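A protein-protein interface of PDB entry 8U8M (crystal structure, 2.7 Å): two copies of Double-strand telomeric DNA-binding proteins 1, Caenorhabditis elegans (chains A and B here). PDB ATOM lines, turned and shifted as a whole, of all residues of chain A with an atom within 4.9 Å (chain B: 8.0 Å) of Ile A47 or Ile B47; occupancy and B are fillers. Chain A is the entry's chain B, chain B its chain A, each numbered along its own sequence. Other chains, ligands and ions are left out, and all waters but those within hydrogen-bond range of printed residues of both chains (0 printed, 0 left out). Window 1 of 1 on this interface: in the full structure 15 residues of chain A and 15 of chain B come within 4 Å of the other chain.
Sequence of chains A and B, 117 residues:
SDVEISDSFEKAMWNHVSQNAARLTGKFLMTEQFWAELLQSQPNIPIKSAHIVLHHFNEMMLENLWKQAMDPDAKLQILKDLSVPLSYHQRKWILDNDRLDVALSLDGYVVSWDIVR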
ATOM      1  N   GLU A   4     -20.276  -0.034 -19.823  1.00  0.00           N
ATOM      2  CA  GLU A   4     -20.613   0.417 -21.173  1.00  0.00           C
ATOM      3  C   GLU A   4     -22.034   0.973 -21.146  1.00  0.00           C
ATOM      4  O   GLU A   4     -23.005   0.214 -21.075  1.00  0.00           O
ATOM      5  CB  GLU A   4     -20.463  -0.722 -22.182  1.00  0.00           C
ATOM      6  CG  GLU A   4     -19.042  -1.269 -22.271  1.00  0.00           C
ATOM      7  CD  GLU A   4     -18.906  -2.421 -23.250  1.00  0.00           C
ATOM      8  OE1 GLU A   4     -19.941  -2.898 -23.762  1.00  0.00           O
ATOM      9  OE2 GLU A   4     -17.760  -2.849 -23.517  1.00  0.00           O
ATOM     10  N   ILE A   5     -22.149   2.300 -21.193  1.00  0.00           N
ATOM     11  CA  ILE A   5     -23.433   2.993 -21.199  1.00  0.00           C
ATOM     12  C   ILE A   5     -23.786   3.354 -22.634  1.00  0.00           C
ATOM     13  O   ILE A   5     -22.962   3.921 -23.361  1.00  0.00           O
ATOM     14  CB  ILE A   5     -23.390   4.251 -20.318  1.00  0.00           C
ATOM     15  CG1 ILE A   5     -23.037   3.891 -18.875  1.00  0.00           C
ATOM     16  CG2 ILE A   5     -24.717   4.977 -20.375  1.00  0.00           C
ATOM     17  CD1 ILE A   5     -24.080   3.032 -18.192  1.00  0.00           C
ATOM     18  N   PHE A   9     -28.953   5.936 -23.388  1.00  0.00           N
ATOM     19  CA  PHE A   9     -29.036   6.125 -21.946  1.00  0.00           C
ATOM     20  C   PHE A   9     -28.320   7.396 -21.508  1.00  0.00           C
ATOM     21  O   PHE A   9     -28.757   8.048 -20.556  1.00  0.00           O
ATOM     22  CB  PHE A   9     -28.483   4.912 -21.201  1.00  0.00           C
ATOM     23  CG  PHE A   9     -28.749   4.954 -19.727  1.00  0.00           C
ATOM     24  CD1 PHE A   9     -30.013   4.694 -19.232  1.00  0.00           C
ATOM     25  CD2 PHE A   9     -27.744   5.286 -18.838  1.00  0.00           C
ATOM     26  CE1 PHE A   9     -30.262   4.753 -17.877  1.00  0.00           C
ATOM     27  CE2 PHE A   9     -27.990   5.342 -17.485  1.00  0.00           C
ATOM     28  CZ  PHE A   9     -29.251   5.076 -17.005  1.00  0.00           C
ATOM     29  N   LEU A  39     -33.485   5.549 -12.806  1.00  0.00           N
ATOM     30  CA  LEU A  39     -33.559   4.108 -13.017  1.00  0.00           C
ATOM     31  C   LEU A  39     -34.940   3.568 -12.667  1.00  0.00           C
ATOM     32  O   LEU A  39     -35.484   2.723 -13.389  1.00  0.00           O
ATOM     33  CB  LEU A  39     -32.474   3.408 -12.202  1.00  0.00           C
ATOM     34  CG  LEU A  39     -31.048   3.608 -12.717  1.00  0.00           C
ATOM     35  CD1 LEU A  39     -30.046   2.967 -11.782  1.00  0.00           C
ATOM     36  CD2 LEU A  39     -30.905   3.045 -14.121  1.00  0.00           C
ATOM     37  N   ILE A  45     -35.317  -2.497 -18.021  1.00  0.00           N
ATOM     38  CA  ILE A  45     -33.870  -2.315 -18.057  1.00  0.00           C
ATOM     39  C   ILE A  45     -33.243  -3.525 -17.375  1.00  0.00           C
ATOM     40  O   ILE A  45     -33.468  -3.734 -16.176  1.00  0.00           O
ATOM     41  CB  ILE A  45     -33.436  -1.009 -17.374  1.00  0.00           C
ATOM     42  CG1 ILE A  45     -34.008   0.197 -18.122  1.00  0.00           C
ATOM     43  CG2 ILE A  45     -31.922  -0.927 -17.306  1.00  0.00           C
ATOM     44  CD1 ILE A  45     -33.611   0.254 -19.586  1.00  0.00           C
ATOM     45  N   PRO A  46     -32.471  -4.350 -18.089  1.00  0.00           N
ATOM     46  CA  PRO A  46     -31.973  -5.589 -17.474  1.00  0.00           C
ATOM     47  C   PRO A  46     -31.033  -5.353 -16.305  1.00  0.00           C
ATOM     48  O   PRO A  46     -31.062  -6.131 -15.343  1.00  0.00           O
ATOM     49  CB  PRO A  46     -31.264  -6.297 -18.637  1.00  0.00           C
ATOM     50  CG  PRO A  46     -30.890  -5.195 -19.573  1.00  0.00           C
ATOM     51  CD  PRO A  46     -31.996  -4.184 -19.473  1.00  0.00           C
ATOM     52  N   ILE A  47     -30.213  -4.306 -16.345  1.00  0.00           N
ATOM     53  CA  ILE A  47     -29.243  -4.025 -15.293  1.00  0.00           C
ATOM     54  C   ILE A  47     -29.438  -2.581 -14.844  1.00  0.00           C
ATOM     55  O   ILE A  47     -29.231  -1.651 -15.632  1.00  0.00           O
ATOM     56  CB  ILE A  47     -27.803  -4.270 -15.764  1.00  0.00           C
ATOM     57  CG1 ILE A  47     -27.694  -5.645 -16.421  1.00  0.00           C
ATOM     58  CG2 ILE A  47     -26.829  -4.165 -14.599  1.00  0.00           C
ATOM     59  CD1 ILE A  47     -26.312  -5.983 -16.927  1.00  0.00           C
ATOM     60  N   LYS A  48     -29.852  -2.391 -13.589  1.00  0.00           N
ATOM     61  CA  LYS A  48     -30.001  -1.065 -12.992  1.00  0.00           C
ATOM     62  C   LYS A  48     -29.101  -0.981 -11.764  1.00  0.00           C
ATOM     63  O   LYS A  48     -29.304  -1.713 -10.790  1.00  0.00           O
ATOM     64  CB  LYS A  48     -31.452  -0.776 -12.602  1.00  0.00           C
ATOM     65  CG  LYS A  48     -32.511  -1.257 -13.583  1.00  0.00           C
ATOM     66  CD  LYS A  48     -33.906  -0.820 -13.134  1.00  0.00           C
ATOM     67  CE  LYS A  48     -35.013  -1.561 -13.887  1.00  0.00           C
ATOM     68  NZ  LYS A  48     -35.090  -3.015 -13.544  1.00  0.00           N
ATOM     69  N   SER A  49     -28.120  -0.081 -11.803  1.00  0.00           N
ATOM     70  CA  SER A  49     -27.267   0.217 -10.656  1.00  0.00           C
ATOM     71  C   SER A  49     -27.076   1.728 -10.583  1.00  0.00           C
ATOM     72  O   SER A  49     -26.433   2.317 -11.457  1.00  0.00           O
ATOM     73  CB  SER A  49     -25.920  -0.499 -10.760  1.00  0.00           C
ATOM     74  OG  SER A  49     -25.090  -0.175  -9.655  1.00  0.00           O
ATOM     75  N   ILE A  52     -23.430   2.677 -10.458  1.00  0.00           N
ATOM     76  CA  ILE A  52     -22.711   2.638 -11.726  1.00  0.00           C
ATOM     77  C   ILE A  52     -23.067   3.841 -12.588  1.00  0.00           C
ATOM     78  O   ILE A  52     -22.199   4.431 -13.241  1.00  0.00           O
ATOM     79  CB  ILE A  52     -22.994   1.310 -12.450  1.00  0.00           C
ATOM     80  CG1 ILE A  52     -22.368   0.150 -11.676  1.00  0.00           C
ATOM     81  CG2 ILE A  52     -22.457   1.350 -13.865  1.00  0.00           C
ATOM     82  CD1 ILE A  52     -20.880   0.314 -11.445  1.00  0.00           C
ATOM     83  N   VAL A  53     -24.344   4.228 -12.598  1.00  0.00           N
ATOM     84  CA  VAL A  53     -24.769   5.395 -13.367  1.00  0.00           C
ATOM     85  C   VAL A  53     -24.129   6.662 -12.813  1.00  0.00           C
ATOM     86  O   VAL A  53     -23.670   7.528 -13.568  1.00  0.00           O
ATOM     87  CB  VAL A  53     -26.306   5.492 -13.370  1.00  0.00           C
ATOM     88  CG1 VAL A  53     -26.757   6.844 -13.893  1.00  0.00           C
ATOM     89  CG2 VAL A  53     -26.906   4.368 -14.198  1.00  0.00           C
ATOM     90  N   ASP B   2     -26.547  -2.135  -5.337  1.00  0.00           N
ATOM     91  CA  ASP B   2     -27.851  -1.604  -5.737  1.00  0.00           C
ATOM     92  C   ASP B   2     -28.231  -2.082  -7.135  1.00  0.00           C
ATOM     93  O   ASP B   2     -28.653  -1.301  -7.986  1.00  0.00           O
ATOM     94  CB  ASP B   2     -27.849  -0.081  -5.657  1.00  0.00           C
ATOM     95  CG  ASP B   2     -26.701   0.549  -6.426  1.00  0.00           C
ATOM     96  OD1 ASP B   2     -25.833  -0.203  -6.927  1.00  0.00           O
ATOM     97  OD2 ASP B   2     -26.664   1.798  -6.526  1.00  0.00           O
ATOM     98  N   VAL B   3     -28.080  -3.382  -7.378  1.00  0.00           N
ATOM     99  CA  VAL B   3     -28.284  -3.978  -8.693  1.00  0.00           C
ATOM    100  C   VAL B   3     -29.639  -4.667  -8.723  1.00  0.00           C
ATOM    101  O   VAL B   3     -30.006  -5.375  -7.777  1.00  0.00           O
ATOM    102  CB  VAL B   3     -27.163  -4.973  -9.035  1.00  0.00           C
ATOM    103  CG1 VAL B   3     -27.343  -5.509 -10.443  1.00  0.00           C
ATOM    104  CG2 VAL B   3     -25.805  -4.313  -8.868  1.00  0.00           C
ATOM    105  N   GLU B   4     -30.378  -4.457  -9.809  1.00  0.00           N
ATOM    106  CA  GLU B   4     -31.667  -5.106 -10.038  1.00  0.00           C
ATOM    107  C   GLU B   4     -31.607  -5.789 -11.400  1.00  0.00           C
ATOM    108  O   GLU B   4     -31.674  -5.122 -12.438  1.00  0.00           O
ATOM    109  CB  GLU B   4     -32.816  -4.102  -9.974  1.00  0.00           C
ATOM    110  CG  GLU B   4     -33.002  -3.460  -8.611  1.00  0.00           C
ATOM    111  CD  GLU B   4     -34.188  -2.516  -8.566  1.00  0.00           C
ATOM    112  OE1 GLU B   4     -34.659  -2.090  -9.642  1.00  0.00           O
ATOM    113  OE2 GLU B   4     -34.651  -2.202  -7.447  1.00  0.00           O
ATOM    114  N   ILE B   5     -31.486  -7.111 -11.394  1.00  0.00           N
ATOM    115  CA  ILE B   5     -31.416  -7.888 -12.623  1.00  0.00           C
ATOM    116  C   ILE B   5     -32.815  -8.366 -12.983  1.00  0.00           C
ATOM    117  O   ILE B   5     -33.502  -8.983 -12.161  1.00  0.00           O
ATOM    118  CB  ILE B   5     -30.453  -9.073 -12.468  1.00  0.00           C
ATOM    119  CG1 ILE B   5     -29.053  -8.582 -12.103  1.00  0.00           C
ATOM    120  CG2 ILE B   5     -30.409  -9.883 -13.750  1.00  0.00           C
ATOM    121  CD1 ILE B   5     -28.327  -7.915 -13.246  1.00  0.00           C
ATOM    122  N   SER B   6     -33.238  -8.082 -14.212  1.00  0.00           N
ATOM    123  CA  SER B   6     -34.542  -8.535 -14.670  1.00  0.00           C
ATOM    124  C   SER B   6     -34.560 -10.053 -14.812  1.00  0.00           C
ATOM    125  O   SER B   6     -33.537 -10.686 -15.092  1.00  0.00           O
ATOM    126  CB  SER B   6     -34.897  -7.881 -16.004  1.00  0.00           C
ATOM    127  OG  SER B   6     -33.974  -8.251 -17.013  1.00  0.00           O
ATOM    128  N   PHE B   9     -33.131 -11.313 -17.935  1.00  0.00           N
ATOM    129  CA  PHE B   9     -31.674 -11.362 -17.968  1.00  0.00           C
ATOM    130  C   PHE B   9     -31.134 -12.512 -17.127  1.00  0.00           C
ATOM    131  O   PHE B   9     -30.106 -13.098 -17.473  1.00  0.00           O
ATOM    132  CB  PHE B   9     -31.073 -10.039 -17.497  1.00  0.00           C
ATOM    133  CG  PHE B   9     -29.599  -9.918 -17.780  1.00  0.00           C
ATOM    134  CD1 PHE B   9     -29.146  -9.777 -19.080  1.00  0.00           C
ATOM    135  CD2 PHE B   9     -28.670  -9.963 -16.752  1.00  0.00           C
ATOM    136  CE1 PHE B   9     -27.797  -9.674 -19.352  1.00  0.00           C
ATOM    137  CE2 PHE B   9     -27.317  -9.859 -17.021  1.00  0.00           C
ATOM    138  CZ  PHE B   9     -26.884  -9.717 -18.322  1.00  0.00           C
ATOM    139  N   MET B  13     -28.766 -15.378 -18.471  1.00  0.00           N
ATOM    140  CA  MET B  13     -27.531 -15.795 -17.812  1.00  0.00           C
ATOM    141  C   MET B  13     -27.491 -17.303 -17.630  1.00  0.00           C
ATOM    142  O   MET B  13     -26.447 -17.933 -17.837  1.00  0.00           O
ATOM    143  CB  MET B  13     -27.391 -15.101 -16.458  1.00  0.00           C
ATOM    144  CG  MET B  13     -27.118 -13.614 -16.533  1.00  0.00           C
ATOM    145  SD  MET B  13     -26.960 -12.860 -14.906  1.00  0.00           S
ATOM    146  CE  MET B  13     -25.515 -13.708 -14.278  1.00  0.00           C
ATOM    147  N   LEU B  38     -20.904 -12.871 -22.502  1.00  0.00           N
ATOM    148  CA  LEU B  38     -22.365 -12.806 -22.547  1.00  0.00           C
ATOM    149  C   LEU B  38     -22.849 -11.423 -22.975  1.00  0.00           C
ATOM    150  O   LEU B  38     -23.694 -11.297 -23.869  1.00  0.00           O
ATOM    151  CB  LEU B  38     -22.958 -13.168 -21.190  1.00  0.00           C
ATOM    152  CG  LEU B  38     -24.473 -12.960 -21.068  1.00  0.00           C
ATOM    153  CD1 LEU B  38     -25.220 -13.770 -22.123  1.00  0.00           C
ATOM    154  CD2 LEU B  38     -24.962 -13.317 -19.676  1.00  0.00           C
ATOM    155  N   LEU B  39     -22.311 -10.374 -22.349  1.00  0.00           N
ATOM    156  CA  LEU B  39     -22.787  -9.016 -22.597  1.00  0.00           C
ATOM    157  C   LEU B  39     -22.504  -8.573 -24.028  1.00  0.00           C
ATOM    158  O   LEU B  39     -23.331  -7.891 -24.644  1.00  0.00           O
ATOM    159  CB  LEU B  39     -22.147  -8.050 -21.600  1.00  0.00           C
ATOM    160  CG  LEU B  39     -22.596  -8.193 -20.144  1.00  0.00           C
ATOM    161  CD1 LEU B  39     -21.795  -7.291 -19.216  1.00  0.00           C
ATOM    162  CD2 LEU B  39     -24.082  -7.907 -20.020  1.00  0.00           C
ATOM    163  N   GLN B  42     -25.380  -9.489 -26.918  1.00  0.00           N
ATOM    164  CA  GLN B  42     -26.600  -8.744 -27.196  1.00  0.00           C
ATOM    165  C   GLN B  42     -26.340  -7.249 -27.093  1.00  0.00           C
ATOM    166  O   GLN B  42     -26.202  -6.725 -25.976  1.00  0.00           O
ATOM    167  CB  GLN B  42     -27.719  -9.161 -26.239  1.00  0.00           C
ATOM    168  CG  GLN B  42     -27.300  -9.333 -24.786  1.00  0.00           C
ATOM    169  CD  GLN B  42     -28.484  -9.609 -23.878  1.00  0.00           C
ATOM    170  OE1 GLN B  42     -29.575  -9.938 -24.346  1.00  0.00           O
ATOM    171  NE2 GLN B  42     -28.274  -9.479 -22.572  1.00  0.00           N
ATOM    172  N   ASN B  44     -27.789  -3.216 -27.737  1.00  0.00           N
ATOM    173  CA  ASN B  44     -29.033  -2.579 -27.300  1.00  0.00           C
ATOM    174  C   ASN B  44     -29.337  -2.898 -25.836  1.00  0.00           C
ATOM    175  O   ASN B  44     -30.493  -3.066 -25.443  1.00  0.00           O
ATOM    176  CB  ASN B  44     -30.211  -2.966 -28.200  1.00  0.00           C
ATOM    177  CG  ASN B  44     -30.094  -2.382 -29.595  1.00  0.00           C
ATOM    178  OD1 ASN B  44     -29.477  -1.335 -29.794  1.00  0.00           O
ATOM    179  ND2 ASN B  44     -30.689  -3.057 -30.569  1.00  0.00           N
ATOM    180  N   ILE B  45     -28.289  -3.003 -25.029  1.00  0.00           N
ATOM    181  CA  ILE B  45     -28.389  -3.060 -23.574  1.00  0.00           C
ATOM    182  C   ILE B  45     -27.822  -1.755 -23.032  1.00  0.00           C
ATOM    183  O   ILE B  45     -26.641  -1.462 -23.257  1.00  0.00           O
ATOM    184  CB  ILE B  45     -27.642  -4.271 -22.992  1.00  0.00           C
ATOM    185  CG1 ILE B  45     -28.318  -5.573 -23.424  1.00  0.00           C
ATOM    186  CG2 ILE B  45     -27.576  -4.179 -21.475  1.00  0.00           C
ATOM    187  CD1 ILE B  45     -29.787  -5.649 -23.064  1.00  0.00           C
ATOM    188  N   PRO B  46     -28.611  -0.940 -22.327  1.00  0.00           N
ATOM    189  CA  PRO B  46     -28.126   0.400 -21.962  1.00  0.00           C
ATOM    190  C   PRO B  46     -26.977   0.382 -20.975  1.00  0.00           C
ATOM    191  O   PRO B  46     -26.115   1.265 -21.039  1.00  0.00           O
ATOM    192  CB  PRO B  46     -29.370   1.074 -21.370  1.00  0.00           C
ATOM    193  CG  PRO B  46     -30.188  -0.059 -20.852  1.00  0.00           C
ATOM    194  CD  PRO B  46     -29.965  -1.202 -21.806  1.00  0.00           C
ATOM    195  N   ILE B  47     -26.930  -0.590 -20.068  1.00  0.00           N
ATOM    196  CA  ILE B  47     -25.907  -0.647 -19.029  1.00  0.00           C
ATOM    197  C   ILE B  47     -25.284  -2.038 -19.039  1.00  0.00           C
ATOM    198  O   ILE B  47     -25.967  -3.029 -18.759  1.00  0.00           O
ATOM    199  CB  ILE B  47     -26.481  -0.306 -17.644  1.00  0.00           C
ATOM    200  CG1 ILE B  47     -27.194   1.049 -17.698  1.00  0.00           C
ATOM    201  CG2 ILE B  47     -25.381  -0.293 -16.594  1.00  0.00           C
ATOM    202  CD1 ILE B  47     -27.887   1.439 -16.416  1.00  0.00           C
ATOM    203  N   LYS B  48     -23.993  -2.104 -19.364  1.00  0.00           N
ATOM    204  CA  LYS B  48     -23.225  -3.346 -19.428  1.00  0.00           C
ATOM    205  C   LYS B  48     -22.054  -3.242 -18.460  1.00  0.00           C
ATOM    206  O   LYS B  48     -21.179  -2.388 -18.634  1.00  0.00           O
ATOM    207  CB  LYS B  48     -22.704  -3.612 -20.840  1.00  0.00           C
ATOM    208  CG  LYS B  48     -23.751  -3.822 -21.916  1.00  0.00           C
ATOM    209  CD  LYS B  48     -23.055  -4.178 -23.221  1.00  0.00           C
ATOM    210  CE  LYS B  48     -24.039  -4.396 -24.352  1.00  0.00           C
ATOM    211  NZ  LYS B  48     -23.341  -4.844 -25.588  1.00  0.00           N
ATOM    212  N   SER B  49     -22.018  -4.114 -17.455  1.00  0.00           N
ATOM    213  CA  SER B  49     -20.857  -4.252 -16.584  1.00  0.00           C
ATOM    214  C   SER B  49     -20.644  -5.727 -16.285  1.00  0.00           C
ATOM    215  O   SER B  49     -21.483  -6.356 -15.631  1.00  0.00           O
ATOM    216  CB  SER B  49     -21.027  -3.462 -15.288  1.00  0.00           C
ATOM    217  OG  SER B  49     -19.895  -3.635 -14.451  1.00  0.00           O
ATOM    218  N   ALA B  50     -19.525  -6.277 -16.761  1.00  0.00           N
ATOM    219  CA  ALA B  50     -19.228  -7.676 -16.484  1.00  0.00           C
ATOM    220  C   ALA B  50     -18.959  -7.903 -15.003  1.00  0.00           C
ATOM    221  O   ALA B  50     -19.304  -8.960 -14.464  1.00  0.00           O
ATOM    222  CB  ALA B  50     -18.036  -8.135 -17.319  1.00  0.00           C
ATOM    223  N   ILE B  52     -20.425  -6.347 -12.501  1.00  0.00           N
ATOM    224  CA  ILE B  52     -21.723  -6.395 -11.835  1.00  0.00           C
ATOM    225  C   ILE B  52     -22.413  -7.726 -12.098  1.00  0.00           C
ATOM    226  O   ILE B  52     -23.008  -8.322 -11.191  1.00  0.00           O
ATOM    227  CB  ILE B  52     -22.590  -5.203 -12.280  1.00  0.00           C
ATOM    228  CG1 ILE B  52     -22.002  -3.900 -11.742  1.00  0.00           C
ATOM    229  CG2 ILE B  52     -24.013  -5.362 -11.798  1.00  0.00           C
ATOM    230  CD1 ILE B  52     -21.877  -3.878 -10.236  1.00  0.00           C
ATOM    231  N   VAL B  53     -22.339  -8.217 -13.336  1.00  0.00           N
ATOM    232  CA  VAL B  53     -22.982  -9.485 -13.676  1.00  0.00           C
ATOM    233  C   VAL B  53     -22.334 -10.638 -12.917  1.00  0.00           C
ATOM    234  O   VAL B  53     -23.023 -11.530 -12.401  1.00  0.00           O
ATOM    235  CB  VAL B  53     -22.932  -9.710 -15.198  1.00  0.00           C
ATOM    236  CG1 VAL B  53     -23.387 -11.111 -15.543  1.00  0.00           C
ATOM    237  CG2 VAL B  53     -23.792  -8.683 -15.909  1.00  0.00           C
ATOM    238  N   HIS B  56     -23.458 -10.531  -9.347  1.00  0.00           N
ATOM    239  CA  HIS B  56     -24.832 -10.984  -9.186  1.00  0.00           C
ATOM    240  C   HIS B  56     -24.926 -12.498  -9.282  1.00  0.00           C
ATOM    241  O   HIS B  56     -25.643 -13.131  -8.502  1.00  0.00           O
ATOM    242  CB  HIS B  56     -25.740 -10.339 -10.226  1.00  0.00           C
ATOM    243  CG  HIS B  56     -27.142 -10.856 -10.182  1.00  0.00           C
ATOM    244  ND1 HIS B  56     -28.043 -10.478  -9.212  1.00  0.00           N
ATOM    245  CD2 HIS B  56     -27.788 -11.747 -10.971  1.00  0.00           C
ATOM    246  CE1 HIS B  56     -29.191 -11.102  -9.413  1.00  0.00           C
ATOM    247  NE2 HIS B  56     -29.062 -11.878 -10.474  1.00  0.00           N
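The side-chain carboxylate (OD1) of Asp B2 sits at hydrogen-bond distance from the side-chain hydroxyl (OG) of Ser A49 (2.8 Å).
N of Glu B4 sits at hydrogen-bond distance from O of Lys A48.
The backbone NH (N) of Ser B6 sits at hydrogen-bond distance from the backbone carbonyl oxygen (O) of Pro A46.
N of Glu A4 lies within hydrogen-bond range of O of Lys B48 (2.8 Å).
The backbone carbonyl oxygen (O) of Glu A4 sits close to the backbone carbonyl oxygen (O) of Pro B46 (3.3 Å).
The backbone carbonyl oxygen (O) of Pro A46 lies close to the backbone carbonyl oxygen (O) of Glu B4, at 3.1 Å.
The backbone carbonyl oxygen (O) of Lys A48 sits close to the backbone carbonyl oxygen (O) of Asp B2, at 2.9 Å.
OG of Ser B6 lies within hydrogen-bond range of N of Phe B9 (3.3 Å).
O of Leu B39 lies within hydrogen-bond range of NZ of Lys B48.
O of Gln B42 lies within hydrogen-bond range of NZ of Lys B48.
NZ of Lys A48 lies within hydrogen-bond range of O of Ile A45, 3.2 Å away.
OG of Ser A49 sits at hydrogen-bond distance from N of Ile A52 (3.4 Å).
Among the printed residues, pairs that only touch across the chains: Ile A5 with Pro B46 (3.2 Å), Lys A48 with Val B3 (3.3 Å), Pro A46 with Ile B5 (3.3 Å), Ile A47 with Ile B47 (3.5 Å), Glu A4 with Ile B47 (3.7 Å), Ile A45 with Pro B46 (3.7 Å), Pro A46 with Ile B45 (3.7 Å), Ile A5 with Ile B47 (3.7 Å), Val A53 with Ile B47 (3.8 Å), Ile A47 with Val B53 (3.8 Å), Ile A47 with Glu B4 (3.9 Å), Pro A46 with Phe B9 (3.9 Å), Phe A9 with Ile B47 (3.9 Å), Phe A9 with Pro B46 (3.9 Å) and Ile A47 with Ile B5 (3.95 Å).
Of the printed residues of chain B, Phe A9 touches Pro B46 (3.9 Å) and Ile B47 (3.9 Å).
Of chain B, only Glu B4, Ile B5, Ser B6, Phe B9 and Ile B45 come within 4 Å of Pro A46.
Printed residues of chain B within 4 Å of Ile A47: Glu B4 (3.9 Å), Ile B5 (3.95 Å), Ile B47 (3.5 Å) and Val B53 (3.8 Å).
Printed residues of chain A within 4 Å of Val B3: Lys A48.
Printed residues of chain A within 4 Å of Ile B5: Pro A46 (3.3 Å) and Ile A47 (3.95 Å).
Ile B47 touches five residues of chain A.
Of the printed residues of chain A, Val B53 touches Ile A47.
The nearest printed residue of chain B that does not touch Ile A47 is Phe B9 (4.01 Å).
The nearest printed residue of chain A that does not touch Asp B2 is Ile A52 (5.2 Å).
Of the 20 printed residues of chain B, 11 touch a printed residue of chain A.
Printed residues of chain B that touch a printed residue of chain A: Asp B2, Val B3, Glu B4, Ile B5, Ser B6, Phe B9, Ile B45, Pro B46, Ile B47, Lys B48 and Val B53.
Hydrophobic or aromatic side chains of chain B that line the printed part of chain A: Ile B5, Phe B9, Ile B45, Pro B46, Ile B47 and Val B53.
Hydrophobic or aromatic side chains of chain A that line the printed part of chain B: Ile A5, Phe A9, Ile A45, Pro A46, Ile A47 and Val A53.
Along chain A the printed residues that touch a printed residue of chain B span positions 4 to 53.
Among the printed residues, 22 pairs touch across the chains.
Among the printed residues, no Asp or Glu carboxylate lies within 4 Å of a Lys or Arg side-chain nitrogen of the other chain.
Glu A4 touches Pro B46, and with the chains exchanged Pro A46 touches Glu B4.
Glu A4 touches Ile B47, and with the chains exchanged Ile A47 touches Glu B4.
Ile A5 touches Ile B47, and with the chains exchanged Ile A47 touches Ile B5.
Phe A9 touches Pro B46, and with the chains exchanged Pro A46 touches Phe B9.
Positions printed for both chains: 4, 5, 9, 39, 45, 46, 47, 48, 49, 52 and 53.
Of the 22 pairs that touch across the chains among the printed residues, 17 have their exchanged pair printed and touching as well.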
